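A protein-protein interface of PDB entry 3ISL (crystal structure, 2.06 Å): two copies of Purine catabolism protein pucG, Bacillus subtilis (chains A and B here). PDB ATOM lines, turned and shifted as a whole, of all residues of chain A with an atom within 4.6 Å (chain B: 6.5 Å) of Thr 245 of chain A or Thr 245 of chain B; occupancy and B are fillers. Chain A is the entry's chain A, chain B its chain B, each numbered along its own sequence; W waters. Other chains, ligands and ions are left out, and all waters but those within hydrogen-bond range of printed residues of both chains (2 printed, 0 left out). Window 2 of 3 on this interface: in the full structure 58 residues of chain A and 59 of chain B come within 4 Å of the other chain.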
ATOM      1  N   GLU A  76     -22.468 -18.105  22.030  1.00  0.00           N
ATOM      2  CA  GLU A  76     -23.522 -17.201  21.658  1.00  0.00           C
ATOM      3  C   GLU A  76     -24.923 -17.687  22.090  1.00  0.00           C
ATOM      4  O   GLU A  76     -25.724 -16.883  22.649  1.00  0.00           O
ATOM      5  CB  GLU A  76     -23.450 -16.857  20.144  1.00  0.00           C
ATOM      6  CG  GLU A  76     -24.535 -15.815  19.708  1.00  0.00           C
ATOM      7  CD  GLU A  76     -24.230 -15.160  18.375  1.00  0.00           C
ATOM      8  OE1 GLU A  76     -25.131 -14.524  17.803  1.00  0.00           O
ATOM      9  OE2 GLU A  76     -23.082 -15.250  17.897  1.00  0.00           O
ATOM     10  N   ARG A 107     -23.963  -7.079  21.383  1.00  0.00           N
ATOM     11  CA  ARG A 107     -24.878  -7.366  20.310  1.00  0.00           C
ATOM     12  C   ARG A 107     -26.249  -7.817  20.822  1.00  0.00           C
ATOM     13  O   ARG A 107     -27.251  -7.496  20.197  1.00  0.00           O
ATOM     14  CB  ARG A 107     -24.253  -8.353  19.292  1.00  0.00           C
ATOM     15  CG  ARG A 107     -23.022  -7.724  18.540  1.00  0.00           C
ATOM     16  CD  ARG A 107     -22.837  -8.330  17.126  1.00  0.00           C
ATOM     17  NE  ARG A 107     -21.538  -8.016  16.499  1.00  0.00           N
ATOM     18  CZ  ARG A 107     -21.220  -8.226  15.204  1.00  0.00           C
ATOM     19  NH1 ARG A 107     -22.104  -8.705  14.317  1.00  0.00           N
ATOM     20  NH2 ARG A 107     -20.004  -7.918  14.774  1.00  0.00           N
ATOM     21  N   TYR A 108     -26.310  -8.506  21.963  1.00  0.00           N
ATOM     22  CA  TYR A 108     -27.636  -8.845  22.541  1.00  0.00           C
ATOM     23  C   TYR A 108     -28.234  -7.757  23.452  1.00  0.00           C
ATOM     24  O   TYR A 108     -29.239  -7.963  24.122  1.00  0.00           O
ATOM     25  CB  TYR A 108     -27.665 -10.258  23.162  1.00  0.00           C
ATOM     26  CG  TYR A 108     -27.619 -11.297  22.061  1.00  0.00           C
ATOM     27  CD1 TYR A 108     -28.794 -11.634  21.355  1.00  0.00           C
ATOM     28  CD2 TYR A 108     -26.410 -11.857  21.643  1.00  0.00           C
ATOM     29  CE1 TYR A 108     -28.773 -12.514  20.281  1.00  0.00           C
ATOM     30  CE2 TYR A 108     -26.374 -12.764  20.593  1.00  0.00           C
ATOM     31  CZ  TYR A 108     -27.605 -13.074  19.896  1.00  0.00           C
ATOM     32  OH  TYR A 108     -27.656 -13.970  18.862  1.00  0.00           O
ATOM     33  N   PRO A 243     -38.708 -13.227  23.893  1.00  0.00           N
ATOM     34  CA  PRO A 243     -37.987 -14.393  23.374  1.00  0.00           C
ATOM     35  C   PRO A 243     -36.504 -14.090  23.106  1.00  0.00           C
ATOM     36  O   PRO A 243     -36.128 -12.939  22.866  1.00  0.00           O
ATOM     37  CB  PRO A 243     -38.708 -14.706  22.049  1.00  0.00           C
ATOM     38  CG  PRO A 243     -39.334 -13.402  21.611  1.00  0.00           C
ATOM     39  CD  PRO A 243     -39.705 -12.709  22.925  1.00  0.00           C
ATOM     40  N   ILE A 244     -35.682 -15.137  23.177  1.00  0.00           N
ATOM     41  CA  ILE A 244     -34.284 -15.123  22.721  1.00  0.00           C
ATOM     42  C   ILE A 244     -34.261 -14.774  21.200  1.00  0.00           C
ATOM     43  O   ILE A 244     -35.034 -15.378  20.401  1.00  0.00           O
ATOM     44  CB  ILE A 244     -33.643 -16.495  23.031  1.00  0.00           C
ATOM     45  CG1 ILE A 244     -33.591 -16.696  24.556  1.00  0.00           C
ATOM     46  CG2 ILE A 244     -32.306 -16.667  22.337  1.00  0.00           C
ATOM     47  CD1 ILE A 244     -33.848 -18.134  25.024  1.00  0.00           C
ATOM     48  N   THR A 245     -33.412 -13.799  20.826  1.00  0.00           N
ATOM     49  CA  THR A 245     -33.349 -13.224  19.451  1.00  0.00           C
ATOM     50  C   THR A 245     -33.007 -14.264  18.346  1.00  0.00           C
ATOM     51  O   THR A 245     -33.670 -14.332  17.289  1.00  0.00           O
ATOM     52  CB  THR A 245     -32.395 -11.980  19.420  1.00  0.00           C
ATOM     53  OG1 THR A 245     -32.820 -11.043  20.420  1.00  0.00           O
ATOM     54  CG2 THR A 245     -32.335 -11.283  18.027  1.00  0.00           C
ATOM     55  N   SER A 246     -32.004 -15.100  18.611  1.00  0.00           N
ATOM     56  CA  SER A 246     -31.723 -16.224  17.719  1.00  0.00           C
ATOM     57  C   SER A 246     -32.723 -17.390  17.936  1.00  0.00           C
ATOM     58  O   SER A 246     -32.805 -17.962  19.038  1.00  0.00           O
ATOM     59  CB  SER A 246     -30.270 -16.694  17.905  1.00  0.00           C
ATOM     60  OG  SER A 246     -29.965 -17.768  17.041  1.00  0.00           O
ATOM     61  N   ASN A 247     -33.504 -17.704  16.901  1.00  0.00           N
ATOM     62  CA  ASN A 247     -34.275 -18.944  16.901  1.00  0.00           C
ATOM     63  C   ASN A 247     -33.371 -20.198  17.007  1.00  0.00           C
ATOM     64  O   ASN A 247     -33.649 -21.114  17.803  1.00  0.00           O
ATOM     65  CB  ASN A 247     -35.167 -19.041  15.642  1.00  0.00           C
ATOM     66  CG  ASN A 247     -35.848 -20.414  15.522  1.00  0.00           C
ATOM     67  OD1 ASN A 247     -36.894 -20.659  16.141  1.00  0.00           O
ATOM     68  ND2 ASN A 247     -35.238 -21.323  14.744  1.00  0.00           N
ATOM     69  N   GLU B  76     -31.090 -18.143   8.905  1.00  0.00           N
ATOM     70  CA  GLU B  76     -31.017 -17.135   9.925  1.00  0.00           C
ATOM     71  C   GLU B  76     -29.878 -16.151   9.652  1.00  0.00           C
ATOM     72  O   GLU B  76     -30.076 -14.943   9.769  1.00  0.00           O
ATOM     73  CB  GLU B  76     -30.899 -17.739  11.323  1.00  0.00           C
ATOM     74  CG  GLU B  76     -30.865 -16.621  12.423  1.00  0.00           C
ATOM     75  CD  GLU B  76     -31.336 -17.079  13.765  1.00  0.00           C
ATOM     76  OE1 GLU B  76     -31.088 -16.336  14.733  1.00  0.00           O
ATOM     77  OE2 GLU B  76     -31.944 -18.171  13.874  1.00  0.00           O
ATOM     78  N   ALA B  80     -30.675 -12.348   9.093  1.00  0.00           N
ATOM     79  CA  ALA B  80     -30.086 -11.494  10.135  1.00  0.00           C
ATOM     80  C   ALA B  80     -29.201 -10.417   9.562  1.00  0.00           C
ATOM     81  O   ALA B  80     -29.113  -9.319  10.106  1.00  0.00           O
ATOM     82  CB  ALA B  80     -29.274 -12.344  11.175  1.00  0.00           C
ATOM     83  N   ILE B  83     -31.875  -7.918   7.580  1.00  0.00           N
ATOM     84  CA  ILE B  83     -32.928  -7.253   8.348  1.00  0.00           C
ATOM     85  C   ILE B  83     -32.470  -6.302   9.457  1.00  0.00           C
ATOM     86  O   ILE B  83     -31.602  -6.623  10.318  1.00  0.00           O
ATOM     87  CB  ILE B  83     -33.981  -8.253   8.926  1.00  0.00           C
ATOM     88  CG1 ILE B  83     -34.722  -8.990   7.793  1.00  0.00           C
ATOM     89  CG2 ILE B  83     -34.957  -7.498   9.850  1.00  0.00           C
ATOM     90  CD1 ILE B  83     -35.488 -10.242   8.272  1.00  0.00           C
ATOM     91  N   GLU B 103     -40.854 -16.416  12.011  1.00  0.00           N
ATOM     92  CA  GLU B 103     -40.239 -16.420  13.358  1.00  0.00           C
ATOM     93  C   GLU B 103     -38.903 -15.707  13.295  1.00  0.00           C
ATOM     94  O   GLU B 103     -38.667 -14.815  14.077  1.00  0.00           O
ATOM     95  CB  GLU B 103     -40.063 -17.843  13.911  1.00  0.00           C
ATOM     96  CG  GLU B 103     -39.709 -17.942  15.416  1.00  0.00           C
ATOM     97  CD  GLU B 103     -40.932 -17.711  16.336  1.00  0.00           C
ATOM     98  OE1 GLU B 103     -42.077 -18.001  15.896  1.00  0.00           O
ATOM     99  OE2 GLU B 103     -40.770 -17.235  17.509  1.00  0.00           O
ATOM    100  N   ILE B 104     -38.038 -16.071  12.346  1.00  0.00           N
ATOM    101  CA  ILE B 104     -36.704 -15.450  12.240  1.00  0.00           C
ATOM    102  C   ILE B 104     -36.783 -13.955  11.962  1.00  0.00           C
ATOM    103  O   ILE B 104     -36.090 -13.159  12.600  1.00  0.00           O
ATOM    104  CB  ILE B 104     -35.797 -16.144  11.152  1.00  0.00           C
ATOM    105  CG1 ILE B 104     -35.527 -17.585  11.561  1.00  0.00           C
ATOM    106  CG2 ILE B 104     -34.456 -15.389  11.058  1.00  0.00           C
ATOM    107  CD1 ILE B 104     -35.049 -18.486  10.434  1.00  0.00           C
ATOM    108  N   ARG B 107     -38.074 -12.041  14.960  1.00  0.00           N
ATOM    109  CA  ARG B 107     -37.010 -12.006  15.973  1.00  0.00           C
ATOM    110  C   ARG B 107     -35.951 -10.944  15.684  1.00  0.00           C
ATOM    111  O   ARG B 107     -35.389 -10.371  16.588  1.00  0.00           O
ATOM    112  CB  ARG B 107     -36.371 -13.379  16.188  1.00  0.00           C
ATOM    113  CG  ARG B 107     -37.139 -14.164  17.244  1.00  0.00           C
ATOM    114  CD  ARG B 107     -36.556 -15.550  17.574  1.00  0.00           C
ATOM    115  NE  ARG B 107     -37.660 -16.442  17.947  1.00  0.00           N
ATOM    116  CZ  ARG B 107     -37.601 -17.402  18.872  1.00  0.00           C
ATOM    117  NH1 ARG B 107     -36.497 -17.622  19.583  1.00  0.00           N
ATOM    118  NH2 ARG B 107     -38.673 -18.150  19.094  1.00  0.00           N
ATOM    119  N   TYR B 108     -35.702 -10.656  14.416  1.00  0.00           N
ATOM    120  CA  TYR B 108     -34.705  -9.628  14.106  1.00  0.00           C
ATOM    121  C   TYR B 108     -35.337  -8.232  13.978  1.00  0.00           C
ATOM    122  O   TYR B 108     -34.714  -7.283  13.553  1.00  0.00           O
ATOM    123  CB  TYR B 108     -33.815 -10.077  12.948  1.00  0.00           C
ATOM    124  CG  TYR B 108     -32.776 -11.097  13.400  1.00  0.00           C
ATOM    125  CD1 TYR B 108     -31.598 -10.674  13.994  1.00  0.00           C
ATOM    126  CD2 TYR B 108     -32.997 -12.479  13.284  1.00  0.00           C
ATOM    127  CE1 TYR B 108     -30.614 -11.595  14.480  1.00  0.00           C
ATOM    128  CE2 TYR B 108     -32.015 -13.428  13.732  1.00  0.00           C
ATOM    129  CZ  TYR B 108     -30.817 -12.959  14.337  1.00  0.00           C
ATOM    130  OH  TYR B 108     -29.820 -13.831  14.784  1.00  0.00           O
ATOM    131  N   GLY B 109     -36.580  -8.122  14.443  1.00  0.00           N
ATOM    132  CA  GLY B 109     -37.302  -6.840  14.497  1.00  0.00           C
ATOM    133  C   GLY B 109     -37.948  -6.333  13.216  1.00  0.00           C
ATOM    134  O   GLY B 109     -38.252  -5.150  13.107  1.00  0.00           O
ATOM    135  N   ARG B 222     -23.324  -2.635   7.019  1.00  0.00           N
ATOM    136  CA  ARG B 222     -23.495  -3.026   8.434  1.00  0.00           C
ATOM    137  C   ARG B 222     -22.288  -3.667   9.146  1.00  0.00           C
ATOM    138  O   ARG B 222     -21.399  -4.254   8.525  1.00  0.00           O
ATOM    139  CB  ARG B 222     -24.715  -3.948   8.583  1.00  0.00           C
ATOM    140  CG  ARG B 222     -26.057  -3.400   8.078  1.00  0.00           C
ATOM    141  CD  ARG B 222     -27.222  -4.441   8.302  1.00  0.00           C
ATOM    142  NE  ARG B 222     -27.521  -4.607   9.737  1.00  0.00           N
ATOM    143  CZ  ARG B 222     -28.365  -5.502  10.260  1.00  0.00           C
ATOM    144  NH1 ARG B 222     -29.005  -6.375   9.493  1.00  0.00           N
ATOM    145  NH2 ARG B 222     -28.536  -5.538  11.574  1.00  0.00           N
ATOM    146  N   ARG B 242     -25.039  -0.001  12.220  1.00  0.00           N
ATOM    147  CA  ARG B 242     -25.571  -1.011  13.172  1.00  0.00           C
ATOM    148  C   ARG B 242     -25.167  -2.451  12.906  1.00  0.00           C
ATOM    149  O   ARG B 242     -25.406  -2.959  11.812  1.00  0.00           O
ATOM    150  CB  ARG B 242     -27.111  -0.946  13.268  1.00  0.00           C
ATOM    151  CG  ARG B 242     -27.737  -1.920  14.295  1.00  0.00           C
ATOM    152  CD  ARG B 242     -29.270  -1.878  14.317  1.00  0.00           C
ATOM    153  NE  ARG B 242     -29.816  -0.558  13.971  1.00  0.00           N
ATOM    154  CZ  ARG B 242     -30.951  -0.038  14.447  1.00  0.00           C
ATOM    155  NH1 ARG B 242     -31.694  -0.696  15.333  1.00  0.00           N
ATOM    156  NH2 ARG B 242     -31.345   1.163  14.040  1.00  0.00           N
ATOM    157  N   PRO B 243     -24.580  -3.111  13.926  1.00  0.00           N
ATOM    158  CA  PRO B 243     -24.245  -4.544  13.969  1.00  0.00           C
ATOM    159  C   PRO B 243     -25.356  -5.502  13.491  1.00  0.00           C
ATOM    160  O   PRO B 243     -26.548  -5.289  13.790  1.00  0.00           O
ATOM    161  CB  PRO B 243     -23.995  -4.787  15.468  1.00  0.00           C
ATOM    162  CG  PRO B 243     -23.503  -3.474  15.982  1.00  0.00           C
ATOM    163  CD  PRO B 243     -24.121  -2.399  15.139  1.00  0.00           C
ATOM    164  N   ILE B 244     -24.957  -6.541  12.749  1.00  0.00           N
ATOM    165  CA  ILE B 244     -25.775  -7.761  12.602  1.00  0.00           C
ATOM    166  C   ILE B 244     -25.843  -8.336  14.035  1.00  0.00           C
ATOM    167  O   ILE B 244     -24.778  -8.512  14.667  1.00  0.00           O
ATOM    168  CB  ILE B 244     -25.073  -8.840  11.681  1.00  0.00           C
ATOM    169  CG1 ILE B 244     -24.586  -8.289  10.315  1.00  0.00           C
ATOM    170  CG2 ILE B 244     -25.872 -10.136  11.609  1.00  0.00           C
ATOM    171  CD1 ILE B 244     -25.617  -7.703   9.413  1.00  0.00           C
ATOM    172  N   THR B 245     -27.051  -8.631  14.544  1.00  0.00           N
ATOM    173  CA  THR B 245     -27.230  -9.087  15.956  1.00  0.00           C
ATOM    174  C   THR B 245     -26.461 -10.404  16.331  1.00  0.00           C
ATOM    175  O   THR B 245     -25.872 -10.520  17.437  1.00  0.00           O
ATOM    176  CB  THR B 245     -28.751  -9.077  16.415  1.00  0.00           C
ATOM    177  OG1 THR B 245     -29.328  -7.793  16.143  1.00  0.00           O
ATOM    178  CG2 THR B 245     -28.924  -9.396  17.929  1.00  0.00           C
ATOM    179  N   SER B 246     -26.407 -11.356  15.403  1.00  0.00           N
ATOM    180  CA  SER B 246     -25.587 -12.545  15.638  1.00  0.00           C
ATOM    181  C   SER B 246     -24.143 -12.442  15.074  1.00  0.00           C
ATOM    182  O   SER B 246     -23.952 -12.438  13.848  1.00  0.00           O
ATOM    183  CB  SER B 246     -26.296 -13.800  15.117  1.00  0.00           C
ATOM    184  OG  SER B 246     -25.444 -14.924  15.215  1.00  0.00           O
ATOM    185  N   ASN B 247     -23.146 -12.386  15.964  1.00  0.00           N
ATOM    186  CA  ASN B 247     -21.717 -12.435  15.570  1.00  0.00           C
ATOM    187  C   ASN B 247     -21.386 -13.679  14.709  1.00  0.00           C
ATOM    188  O   ASN B 247     -20.697 -13.590  13.675  1.00  0.00           O
ATOM    189  CB  ASN B 247     -20.794 -12.360  16.822  1.00  0.00           C
ATOM    190  CG  ASN B 247     -19.318 -12.669  16.499  1.00  0.00           C
ATOM    191  OD1 ASN B 247     -18.573 -11.795  16.038  1.00  0.00           O
ATOM    192  ND2 ASN B 247     -18.898 -13.925  16.746  1.00  0.00           N
ATOM    193  N   TYR B 248     -21.905 -14.829  15.128  1.00  0.00           N
ATOM    194  CA  TYR B 248     -21.592 -16.108  14.459  1.00  0.00           C
ATOM    195  C   TYR B 248     -22.268 -16.182  13.089  1.00  0.00           C
ATOM    196  O   TYR B 248     -21.732 -16.809  12.176  1.00  0.00           O
ATOM    197  CB  TYR B 248     -21.965 -17.293  15.360  1.00  0.00           C
ATOM    198  CG  TYR B 248     -21.697 -18.655  14.799  1.00  0.00           C
ATOM    199  CD1 TYR B 248     -20.491 -19.322  15.091  1.00  0.00           C
ATOM    200  CD2 TYR B 248     -22.653 -19.309  14.016  1.00  0.00           C
ATOM    201  CE1 TYR B 248     -20.243 -20.590  14.600  1.00  0.00           C
ATOM    202  CE2 TYR B 248     -22.413 -20.579  13.488  1.00  0.00           C
ATOM    203  CZ  TYR B 248     -21.216 -21.219  13.794  1.00  0.00           C
ATOM    204  OH  TYR B 248     -20.973 -22.480  13.311  1.00  0.00           O
HETATM  205  O   HOH W   1     -32.822 -20.532  12.890  1.00  0.00           O
HETATM  206  O   HOH W   2     -20.486 -16.123  17.970  1.00  0.00           O
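Glu 76 of chain A touches Ser 246 of chain B, and with the chains exchanged Ser 246 of chain A touches Glu 76 of chain B.
Glu 76 of chain A touches Asn 247 of chain B, and with the chains exchanged Asn 247 of chain A touches Glu 76 of chain B.
Arg 107 of chain A touches Ile 244 of chain B, and with the chains exchanged Ile 244 of chain A touches Arg 107 of chain B.
Tyr 108 of chain A touches Ser 246 of chain B, but with the chains exchanged Ser 246 of chain A does not touch Tyr 108 of chain B (4.2 Å).
8 positions are printed for both chains.
N of Asn 247 of chain A sits at hydrogen-bond distance from OE2 of Glu 76 of chain B (3.4 Å).
The backbone NH (N) of Tyr 248 of chain B lies within hydrogen-bond range of the side-chain carboxylate (OE2) of Glu 76 of chain A (3.0 Å).
NH1 of Arg 107 of chain B lies within hydrogen-bond range of O of Ile 244 of chain A.
The backbone carbonyl oxygen (O) of Ile 244 of chain B is in hydrogen-bond range of the guanidinium group (NH1) of Arg 107 of chain A.
OE1 of Glu 76 of chain A lies within hydrogen-bond range of OG of Ser 246 of chain B (2.6 Å).
OG of Ser 246 of chain A is in hydrogen-bond range of OE1 of Glu 76 of chain B, 2.9 Å away.
The backbone NH of Asn 247 of chain B is in hydrogen-bond range of the side-chain carboxylate of Glu 76 of chain A.
Of the printed residues of chain B, Thr 245 of chain A touches Arg 107, Tyr 108 and Thr 245.
Printed residues of chain A within 4 Å of Glu 76 of chain B: Ser 246 (2.9 Å) and Asn 247 (3.4 Å).
Printed residues of chain B within 4 Å of Ser 246 of chain A: Glu 76 (2.9 Å) and Arg 107 (3.7 Å).
Of the printed residues of chain B, Asn 247 of chain A touches Glu 76 (3.4 Å), Glu 103 (3.98 Å) and Arg 107 (3.7 Å).
Of the printed residues of chain B, Tyr 108 of chain A touches Thr 245 (3.9 Å) and Ser 246 (3.99 Å).
The nearest residue of chain A that does not touch Thr 245 of chain B is Glu 76 of chain A (4.1 Å).
Water W1 bridges OE2 of Glu 76 of chain B and ND2 of Asn 247 of chain A.
Water W2 lies within hydrogen-bond range of OE2 of Glu 76 of chain A (2.7 Å), ND2 of Asn 247 of chain B (3.0 Å) and N of Tyr 248 of chain B (3.4 Å).
The side-chain carboxylate (OE1) of Glu 76 of chain B is in hydrogen-bond range of the side-chain hydroxyl (OH) of Tyr 108 of chain B, 2.8 Å away.
NH2 of Arg 107 of chain B is in salt-bridge range of OE2 of Glu 103 of chain B.
The side-chain hydroxyl (OH) of Tyr 108 of chain A sits at hydrogen-bond distance from the side-chain carboxylate (OE1) of Glu 76 of chain A, 2.8 Å away.
Of the 8 printed residues of chain A, 7 touch a printed residue of chain B.
Hydrophobic or aromatic side chains of chain A within 4 Å of the printed part of chain B: Tyr 108.
Of the 16 printed residues of chain B, 9 touch a printed residue of chain A.
Hydrophobic or aromatic side chains of chain B that line the printed part of chain A: Tyr 108, Ile 244 and Tyr 248.
Among the printed residues, 17 pairs touch across the chains.
Among the printed residues, no Asp or Glu carboxylate lies within 4 Å of a Lys or Arg side-chain nitrogen of the other chain.
Among the printed residues, merely in contact across the chains: Thr 245 of chain A with Arg 107 of chain B (3.1 Å), Arg 107 of chain A with Thr 245 of chain B (3.3 Å), Asn 247 of chain A with Arg 107 of chain B (3.7 Å), Ser 246 of chain A with Arg 107 of chain B (3.7 Å), Thr 245 of chain A with Thr 245 of chain B (3.9 Å), Tyr 108 of chain A with Thr 245 of chain B (3.9 Å), Arg 107 of chain A with Asn 247 of chain B (3.95 Å), Thr 245 of chain A with Tyr 108 of chain B (3.95 Å), Asn 247 of chain A with Glu 103 of chain B (3.98 Å) and Tyr 108 of chain A with Ser 246 of chain B (3.99 Å).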
